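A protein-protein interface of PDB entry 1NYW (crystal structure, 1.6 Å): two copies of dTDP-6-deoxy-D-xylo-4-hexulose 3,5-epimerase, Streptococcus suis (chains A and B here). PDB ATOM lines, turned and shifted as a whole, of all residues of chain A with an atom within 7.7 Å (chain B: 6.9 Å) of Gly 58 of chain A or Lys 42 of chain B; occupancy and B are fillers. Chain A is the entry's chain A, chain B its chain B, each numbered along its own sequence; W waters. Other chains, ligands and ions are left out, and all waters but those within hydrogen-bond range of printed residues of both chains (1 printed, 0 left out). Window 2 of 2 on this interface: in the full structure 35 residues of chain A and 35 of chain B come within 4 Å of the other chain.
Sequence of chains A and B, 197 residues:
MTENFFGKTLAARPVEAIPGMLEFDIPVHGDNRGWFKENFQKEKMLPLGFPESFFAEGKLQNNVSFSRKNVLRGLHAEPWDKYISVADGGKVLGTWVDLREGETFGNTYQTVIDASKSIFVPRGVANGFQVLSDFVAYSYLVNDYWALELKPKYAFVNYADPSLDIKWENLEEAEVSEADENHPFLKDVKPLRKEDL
The backbone carbonyl oxygen of Phe 40 of chain B sits at hydrogen-bond distance from the backbone NH of Asn 62 of chain A (2.8 Å). O of Leu 60 of chain A lies within hydrogen-bond range of N of Lys 42 of chain B, at 3.2 Å. NZ of Lys 42 of chain B is in hydrogen-bond range of O of Gly 58 of chain A, at 2.6 Å.
Gly 58 of chain A touches just one residue of chain B: Lys 42. Printed residues of chain A within 4 Å of Lys 42 of chain B: Gly 58, Leu 60 and Tyr 145. Of the printed residues of chain A, Phe 40 of chain B touches Leu 60 (3.7 Å), Gln 61 (3.2 Å) and Asn 62 (2.8 Å). Printed residues of chain B within 4 Å of Leu 60 of chain A: Phe 40 (3.7 Å), Lys 42 (3.2 Å) and Phe 55 (3.9 Å). Printed residues of chain B within 4 Å of Gln 61 of chain A: Phe 40 (3.2 Å) and Gln 41 (3.5 Å). Printed residues of chain B within 4 Å of Asn 62 of chain A: Phe 40. Lys 59 of chain A touches none of the printed residues of chain B. The nearest printed residue of chain B that does not touch Gln 61 of chain A is Lys 42 of chain B (5.0 Å).
Water W1 lies within hydrogen-bond range of the side-chain amide nitrogen (NE2) of Gln 41 of chain B (3.0 Å) and the side-chain amide oxygen (OE1) of Gln 61 of chain A (3.3 Å).
Among the printed residues, merely in contact across the chains: Gln 61 of chain A with Phe 40 of chain B (3.2 Å), Tyr 145 of chain A with Lys 42 of chain B (3.4 Å), Tyr 145 of chain A with Gln 41 of chain B (3.5 Å), Gln 61 of chain A with Gln 41 of chain B (3.5 Å), Tyr 145 of chain A with Glu 43 of chain B (3.6 Å), Leu 60 of chain A with Phe 40 of chain B (3.7 Å) and Leu 60 of chain A with Phe 55 of chain B (3.9 Å).
1 position is printed for both chains. Of the 10 pairs that touch across the chains among the printed residues, none has its exchanged pair printed and touching as well.
Of the 11 printed residues of chain B, 5 touch a printed residue of chain A. Hydrophobic or aromatic side chains of chain B that line the printed part of chain A: Phe 40 and Phe 55. Along chain A the printed residues that touch a printed residue of chain B span positions 58 to 145. Among the printed residues, 10 pairs touch across the chains. Among the printed residues, no Asp or Glu carboxylate lies within 4 Å of a Lys or Arg side-chain nitrogen of the other chain.
The backbone NH of Glu 43 of chain B is in hydrogen-bond range of the side-chain amide oxygen of Gln 41 of chain B, 2.9 Å away. The backbone NH (N) of Val 142 of chain A sits at hydrogen-bond distance from the backbone carbonyl oxygen (O) of Gln 61 of chain A, at 2.9 Å. The backbone NH of Lys 44 of chain B is in hydrogen-bond range of the side-chain amide oxygen of Gln 41 of chain B, 2.9 Å away. N of Gln 41 of chain B is in hydrogen-bond range of SD of Met 45 of chain B. The side-chain hydroxyl (OH) of Tyr 145 of chain A is in hydrogen-bond range of the backbone NH (N) of Leu 60 of chain A (3.2 Å).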
ATOM      1  N   SER A  53      20.849  17.539  -0.224  1.00  0.00           N
ATOM      2  CA  SER A  53      19.840  17.092  -1.179  1.00  0.00           C
ATOM      3  C   SER A  53      20.069  15.617  -1.549  1.00  0.00           C
ATOM      4  O   SER A  53      19.216  14.989  -2.186  1.00  0.00           O
ATOM      5  CB  SER A  53      19.916  17.927  -2.443  1.00  0.00           C
ATOM      6  OG  SER A  53      21.099  17.626  -3.173  1.00  0.00           O
ATOM      7  N   PHE A  54      21.242  15.111  -1.193  1.00  0.00           N
ATOM      8  CA  PHE A  54      21.562  13.706  -1.451  1.00  0.00           C
ATOM      9  C   PHE A  54      20.594  12.685  -0.832  1.00  0.00           C
ATOM     10  O   PHE A  54      20.234  11.745  -1.505  1.00  0.00           O
ATOM     11  CB  PHE A  54      23.001  13.355  -0.998  1.00  0.00           C
ATOM     12  CG  PHE A  54      23.460  11.972  -1.411  1.00  0.00           C
ATOM     13  CD1 PHE A  54      23.988  11.733  -2.659  1.00  0.00           C
ATOM     14  CD2 PHE A  54      23.302  10.867  -0.542  1.00  0.00           C
ATOM     15  CE1 PHE A  54      24.404  10.423  -3.023  1.00  0.00           C
ATOM     16  CE2 PHE A  54      23.723   9.575  -0.907  1.00  0.00           C
ATOM     17  CZ  PHE A  54      24.251   9.373  -2.136  1.00  0.00           C
ATOM     18  N   PHE A  55      20.240  12.862   0.440  1.00  0.00           N
ATOM     19  CA  PHE A  55      19.412  11.924   1.209  1.00  0.00           C
ATOM     20  C   PHE A  55      17.921  12.240   1.310  1.00  0.00           C
ATOM     21  O   PHE A  55      17.186  11.503   1.970  1.00  0.00           O
ATOM     22  CB  PHE A  55      19.895  11.896   2.652  1.00  0.00           C
ATOM     23  CG  PHE A  55      21.319  11.564   2.777  1.00  0.00           C
ATOM     24  CD1 PHE A  55      21.724  10.244   2.771  1.00  0.00           C
ATOM     25  CD2 PHE A  55      22.277  12.577   2.837  1.00  0.00           C
ATOM     26  CE1 PHE A  55      23.061   9.914   2.852  1.00  0.00           C
ATOM     27  CE2 PHE A  55      23.620  12.244   2.932  1.00  0.00           C
ATOM     28  CZ  PHE A  55      23.992  10.920   2.930  1.00  0.00           C
ATOM     29  N   ALA A  56      17.493  13.257   0.607  1.00  0.00           N
ATOM     30  CA  ALA A  56      16.163  13.847   0.879  1.00  0.00           C
ATOM     31  C   ALA A  56      14.983  13.021   0.345  1.00  0.00           C
ATOM     32  O   ALA A  56      13.885  13.110   0.898  1.00  0.00           O
ATOM     33  CB  ALA A  56      16.093  15.247   0.369  1.00  0.00           C
ATOM     34  N   GLU A  57      15.205  12.155  -0.656  1.00  0.00           N
ATOM     35  CA  GLU A  57      14.149  11.202  -1.062  1.00  0.00           C
ATOM     36  C   GLU A  57      14.136   9.961  -0.177  1.00  0.00           C
ATOM     37  O   GLU A  57      13.297   9.093  -0.363  1.00  0.00           O
ATOM     38  CB  GLU A  57      14.326  10.737  -2.508  1.00  0.00           C
ATOM     39  CG  GLU A  57      14.180  11.782  -3.607  1.00  0.00           C
ATOM     40  CD  GLU A  57      14.363  11.162  -4.991  1.00  0.00           C
ATOM     41  OE1 GLU A  57      13.680  10.166  -5.301  1.00  0.00           O
ATOM     42  OE2 GLU A  57      15.189  11.652  -5.795  1.00  0.00           O
ATOM     43  N   GLY A  58      15.077   9.876   0.760  1.00  0.00           N
ATOM     44  CA  GLY A  58      15.168   8.772   1.679  1.00  0.00           C
ATOM     45  C   GLY A  58      15.592   7.466   1.011  1.00  0.00           C
ATOM     46  O   GLY A  58      15.373   6.412   1.569  1.00  0.00           O
ATOM     47  N   LYS A  59      16.189   7.537  -0.170  1.00  0.00           N
ATOM     48  CA  LYS A  59      16.612   6.339  -0.868  1.00  0.00           C
ATOM     49  C   LYS A  59      18.114   6.106  -0.614  1.00  0.00           C
ATOM     50  O   LYS A  59      18.877   7.079  -0.532  1.00  0.00           O
ATOM     51  CB  LYS A  59      16.365   6.514  -2.364  1.00  0.00           C
ATOM     52  CG  LYS A  59      14.882   6.825  -2.743  1.00  0.00           C
ATOM     53  CD  LYS A  59      14.734   7.042  -4.224  1.00  0.00           C
ATOM     54  CE  LYS A  59      13.263   6.873  -4.655  1.00  0.00           C
ATOM     55  NZ  LYS A  59      13.147   7.291  -6.089  1.00  0.00           N
ATOM     56  N   LEU A  60      18.522   4.857  -0.459  1.00  0.00           N
ATOM     57  CA  LEU A  60      19.917   4.608  -0.211  1.00  0.00           C
ATOM     58  C   LEU A  60      20.303   3.207  -0.745  1.00  0.00           C
ATOM     59  O   LEU A  60      19.619   2.250  -0.511  1.00  0.00           O
ATOM     60  CB  LEU A  60      20.297   4.650   1.278  1.00  0.00           C
ATOM     61  CG  LEU A  60      21.844   4.433   1.538  1.00  0.00           C
ATOM     62  CD1 LEU A  60      22.715   5.668   1.097  1.00  0.00           C
ATOM     63  CD2 LEU A  60      22.140   4.090   2.952  1.00  0.00           C
ATOM     64  N   GLN A  61      21.417   3.165  -1.460  1.00  0.00           N
ATOM     65  CA  GLN A  61      21.933   1.888  -1.949  1.00  0.00           C
ATOM     66  C   GLN A  61      23.462   1.983  -1.953  1.00  0.00           C
ATOM     67  O   GLN A  61      23.993   3.019  -2.212  1.00  0.00           O
ATOM     68  CB  GLN A  61      21.431   1.637  -3.359  1.00  0.00           C
ATOM     69  CG  GLN A  61      22.056   0.485  -4.109  1.00  0.00           C
ATOM     70  CD  GLN A  61      21.445   0.174  -5.478  1.00  0.00           C
ATOM     71  OE1 GLN A  61      20.409   0.724  -5.845  1.00  0.00           O
ATOM     72  NE2 GLN A  61      22.014  -0.656  -6.247  1.00  0.00           N
ATOM     73  N   ASN A  62      24.121   0.911  -1.573  1.00  0.00           N
ATOM     74  CA  ASN A  62      25.584   0.837  -1.500  1.00  0.00           C
ATOM     75  C   ASN A  62      25.985  -0.341  -2.427  1.00  0.00           C
ATOM     76  O   ASN A  62      25.562  -1.460  -2.182  1.00  0.00           O
ATOM     77  CB  ASN A  62      26.028   0.533  -0.045  1.00  0.00           C
ATOM     78  CG  ASN A  62      27.542   0.156   0.084  1.00  0.00           C
ATOM     79  OD1 ASN A  62      27.930  -0.573   0.965  1.00  0.00           O
ATOM     80  ND2 ASN A  62      28.416   0.768  -0.758  1.00  0.00           N
ATOM     81  N   VAL A 142      24.625   5.571  -3.476  1.00  0.00           N
ATOM     82  CA  VAL A 142      23.750   6.190  -4.457  1.00  0.00           C
ATOM     83  C   VAL A 142      22.382   6.472  -3.819  1.00  0.00           C
ATOM     84  O   VAL A 142      22.022   5.863  -2.825  1.00  0.00           O
ATOM     85  CB  VAL A 142      23.582   5.419  -5.746  1.00  0.00           C
ATOM     86  CG1 VAL A 142      24.897   5.100  -6.367  1.00  0.00           C
ATOM     87  CG2 VAL A 142      22.806   4.098  -5.502  1.00  0.00           C
ATOM     88  N   ASN A 143      21.663   7.401  -4.443  1.00  0.00           N
ATOM     89  CA  ASN A 143      20.390   7.881  -3.907  1.00  0.00           C
ATOM     90  C   ASN A 143      19.183   7.634  -4.797  1.00  0.00           C
ATOM     91  O   ASN A 143      18.152   8.322  -4.638  1.00  0.00           O
ATOM     92  CB  ASN A 143      20.483   9.334  -3.483  1.00  0.00           C
ATOM     93  CG  ASN A 143      20.874  10.246  -4.637  1.00  0.00           C
ATOM     94  OD1 ASN A 143      21.050   9.776  -5.720  1.00  0.00           O
ATOM     95  ND2 ASN A 143      20.894  11.575  -4.399  1.00  0.00           N
ATOM     96  N   TYR A 145      17.491   4.041  -7.384  1.00  0.00           N
ATOM     97  CA  TYR A 145      17.593   2.600  -7.577  1.00  0.00           C
ATOM     98  C   TYR A 145      17.589   2.181  -9.035  1.00  0.00           C
ATOM     99  O   TYR A 145      16.659   2.480  -9.791  1.00  0.00           O
ATOM    100  CB  TYR A 145      16.422   1.942  -6.841  1.00  0.00           C
ATOM    101  CG  TYR A 145      16.317   2.277  -5.374  1.00  0.00           C
ATOM    102  CD1 TYR A 145      15.163   2.831  -4.860  1.00  0.00           C
ATOM    103  CD2 TYR A 145      17.380   2.039  -4.493  1.00  0.00           C
ATOM    104  CE1 TYR A 145      15.075   3.171  -3.539  1.00  0.00           C
ATOM    105  CE2 TYR A 145      17.262   2.304  -3.153  1.00  0.00           C
ATOM    106  CZ  TYR A 145      16.104   2.869  -2.690  1.00  0.00           C
ATOM    107  OH  TYR A 145      15.941   3.192  -1.389  1.00  0.00           O
ATOM    108  N   PHE B  40      23.921  -3.132  -0.137  1.00  0.00           N
ATOM    109  CA  PHE B  40      22.774  -2.665   0.630  1.00  0.00           C
ATOM    110  C   PHE B  40      21.806  -1.968  -0.338  1.00  0.00           C
ATOM    111  O   PHE B  40      22.230  -1.177  -1.145  1.00  0.00           O
ATOM    112  CB  PHE B  40      23.102  -1.685   1.772  1.00  0.00           C
ATOM    113  CG  PHE B  40      21.857  -1.171   2.452  1.00  0.00           C
ATOM    114  CD1 PHE B  40      21.203  -1.978   3.322  1.00  0.00           C
ATOM    115  CD2 PHE B  40      21.318   0.078   2.141  1.00  0.00           C
ATOM    116  CE1 PHE B  40      20.083  -1.601   3.917  1.00  0.00           C
ATOM    117  CE2 PHE B  40      20.185   0.504   2.745  1.00  0.00           C
ATOM    118  CZ  PHE B  40      19.545  -0.336   3.629  1.00  0.00           C
ATOM    119  N   GLN B  41      20.504  -2.246  -0.227  1.00  0.00           N
ATOM    120  CA  GLN B  41      19.556  -1.697  -1.168  1.00  0.00           C
ATOM    121  C   GLN B  41      18.255  -1.561  -0.338  1.00  0.00           C
ATOM    122  O   GLN B  41      17.619  -2.499  -0.082  1.00  0.00           O
ATOM    123  CB  GLN B  41      19.369  -2.529  -2.443  1.00  0.00           C
ATOM    124  CG  GLN B  41      19.066  -1.823  -3.772  1.00  0.00           C
ATOM    125  CD  GLN B  41      17.594  -1.505  -3.919  1.00  0.00           C
ATOM    126  OE1 GLN B  41      16.876  -1.415  -2.907  1.00  0.00           O
ATOM    127  NE2 GLN B  41      17.118  -1.350  -5.143  1.00  0.00           N
ATOM    128  N   LYS B  42      17.954  -0.358   0.092  1.00  0.00           N
ATOM    129  CA  LYS B  42      16.865  -0.120   1.027  1.00  0.00           C
ATOM    130  C   LYS B  42      15.549  -0.651   0.513  1.00  0.00           C
ATOM    131  O   LYS B  42      14.771  -1.225   1.270  1.00  0.00           O
ATOM    132  CB  LYS B  42      16.777   1.380   1.352  1.00  0.00           C
ATOM    133  CG  LYS B  42      15.781   1.711   2.410  1.00  0.00           C
ATOM    134  CD  LYS B  42      15.771   3.237   2.701  1.00  0.00           C
ATOM    135  CE  LYS B  42      14.639   3.606   3.559  1.00  0.00           C
ATOM    136  NZ  LYS B  42      14.416   5.097   3.568  1.00  0.00           N
ATOM    137  N   GLU B  43      15.206  -0.342  -0.732  1.00  0.00           N
ATOM    138  CA  GLU B  43      13.882  -0.674  -1.243  1.00  0.00           C
ATOM    139  C   GLU B  43      13.681  -2.183  -1.319  1.00  0.00           C
ATOM    140  O   GLU B  43      12.611  -2.664  -1.004  1.00  0.00           O
ATOM    141  CB  GLU B  43      13.691   0.003  -2.609  1.00  0.00           C
ATOM    142  CG  GLU B  43      12.348  -0.240  -3.279  1.00  0.00           C
ATOM    143  CD  GLU B  43      12.064   0.769  -4.380  1.00  0.00           C
ATOM    144  OE1 GLU B  43      12.392   0.502  -5.547  1.00  0.00           O
ATOM    145  OE2 GLU B  43      11.501   1.838  -4.072  1.00  0.00           O
ATOM    146  N   LYS B  44      14.745  -2.887  -1.675  1.00  0.00           N
ATOM    147  CA  LYS B  44      14.629  -4.353  -1.740  1.00  0.00           C
ATOM    148  C   LYS B  44      14.782  -5.070  -0.401  1.00  0.00           C
ATOM    149  O   LYS B  44      14.359  -6.190  -0.258  1.00  0.00           O
ATOM    150  CB  LYS B  44      15.712  -4.923  -2.639  1.00  0.00           C
ATOM    151  CG  LYS B  44      15.526  -4.638  -4.115  1.00  0.00           C
ATOM    152  CD  LYS B  44      16.695  -5.129  -4.941  1.00  0.00           C
ATOM    153  CE  LYS B  44      16.600  -4.583  -6.372  1.00  0.00           C
ATOM    154  NZ  LYS B  44      17.708  -5.126  -7.284  1.00  0.00           N
ATOM    155  N   MET B  45      15.423  -4.424   0.553  1.00  0.00           N
ATOM    156  CA  MET B  45      15.762  -5.099   1.815  1.00  0.00           C
ATOM    157  C   MET B  45      14.742  -4.794   2.938  1.00  0.00           C
ATOM    158  O   MET B  45      14.551  -5.668   3.861  1.00  0.00           O
ATOM    159  CB  MET B  45      17.195  -4.727   2.223  1.00  0.00           C
ATOM    160  CG  MET B  45      18.226  -5.437   1.337  1.00  0.00           C
ATOM    161  SD  MET B  45      19.844  -5.030   1.768  1.00  0.00           S
ATOM    162  CE  MET B  45      20.743  -6.072   0.648  1.00  0.00           C
ATOM    163  N   LEU B  46      14.074  -3.626   2.913  1.00  0.00           N
ATOM    164  CA  LEU B  46      12.979  -3.365   3.885  1.00  0.00           C
ATOM    165  C   LEU B  46      11.943  -4.503   3.937  1.00  0.00           C
ATOM    166  O   LEU B  46      11.640  -5.006   5.031  1.00  0.00           O
ATOM    167  CB  LEU B  46      12.271  -2.000   3.638  1.00  0.00           C
ATOM    168  CG  LEU B  46      12.992  -0.709   4.070  1.00  0.00           C
ATOM    169  CD1 LEU B  46      12.110   0.563   3.931  1.00  0.00           C
ATOM    170  CD2 LEU B  46      13.515  -0.805   5.478  1.00  0.00           C
ATOM    171  N   PRO B  47      11.408  -4.916   2.790  1.00  0.00           N
ATOM    172  CA  PRO B  47      10.436  -6.013   2.750  1.00  0.00           C
ATOM    173  C   PRO B  47      10.942  -7.359   3.285  1.00  0.00           C
ATOM    174  O   PRO B  47      10.144  -8.207   3.654  1.00  0.00           O
ATOM    175  CB  PRO B  47      10.073  -6.126   1.279  1.00  0.00           C
ATOM    176  CG  PRO B  47      10.634  -4.938   0.607  1.00  0.00           C
ATOM    177  CD  PRO B  47      11.689  -4.372   1.433  1.00  0.00           C
ATOM    178  N   PHE B  50      14.787  -5.815   6.932  1.00  0.00           N
ATOM    179  CA  PHE B  50      15.722  -4.757   7.339  1.00  0.00           C
ATOM    180  C   PHE B  50      14.895  -3.655   8.004  1.00  0.00           C
ATOM    181  O   PHE B  50      13.919  -3.180   7.407  1.00  0.00           O
ATOM    182  CB  PHE B  50      16.567  -4.222   6.179  1.00  0.00           C
ATOM    183  CG  PHE B  50      17.667  -3.313   6.624  1.00  0.00           C
ATOM    184  CD1 PHE B  50      18.944  -3.766   6.834  1.00  0.00           C
ATOM    185  CD2 PHE B  50      17.419  -1.975   6.826  1.00  0.00           C
ATOM    186  CE1 PHE B  50      19.925  -2.917   7.287  1.00  0.00           C
ATOM    187  CE2 PHE B  50      18.379  -1.135   7.286  1.00  0.00           C
ATOM    188  CZ  PHE B  50      19.659  -1.611   7.480  1.00  0.00           C
ATOM    189  N   GLU B  52      12.983  -0.464   9.382  1.00  0.00           N
ATOM    190  CA  GLU B  52      12.756   0.914   8.968  1.00  0.00           C
ATOM    191  C   GLU B  52      13.340   1.937   9.935  1.00  0.00           C
ATOM    192  O   GLU B  52      13.739   3.029   9.521  1.00  0.00           O
ATOM    193  CB  GLU B  52      11.255   1.169   8.895  1.00  0.00           C
ATOM    194  CG  GLU B  52      10.705   0.979   7.512  1.00  0.00           C
ATOM    195  CD  GLU B  52       9.311   1.556   7.366  1.00  0.00           C
ATOM    196  OE1 GLU B  52       8.539   1.555   8.372  1.00  0.00           O
ATOM    197  OE2 GLU B  52       8.993   2.000   6.240  1.00  0.00           O
ATOM    198  N   PHE B  55      16.846   4.115   9.683  1.00  0.00           N
ATOM    199  CA  PHE B  55      16.920   5.425   8.980  1.00  0.00           C
ATOM    200  C   PHE B  55      16.162   6.597   9.560  1.00  0.00           C
ATOM    201  O   PHE B  55      16.256   7.716   9.039  1.00  0.00           O
ATOM    202  CB  PHE B  55      16.398   5.247   7.569  1.00  0.00           C
ATOM    203  CG  PHE B  55      17.219   4.340   6.777  1.00  0.00           C
ATOM    204  CD1 PHE B  55      16.846   3.020   6.610  1.00  0.00           C
ATOM    205  CD2 PHE B  55      18.411   4.774   6.244  1.00  0.00           C
ATOM    206  CE1 PHE B  55      17.652   2.151   5.882  1.00  0.00           C
ATOM    207  CE2 PHE B  55      19.192   3.925   5.521  1.00  0.00           C
ATOM    208  CZ  PHE B  55      18.821   2.612   5.353  1.00  0.00           C
HETATM  209  O   HOH W   1      18.828  -1.518  -7.608  1.00  0.00           O
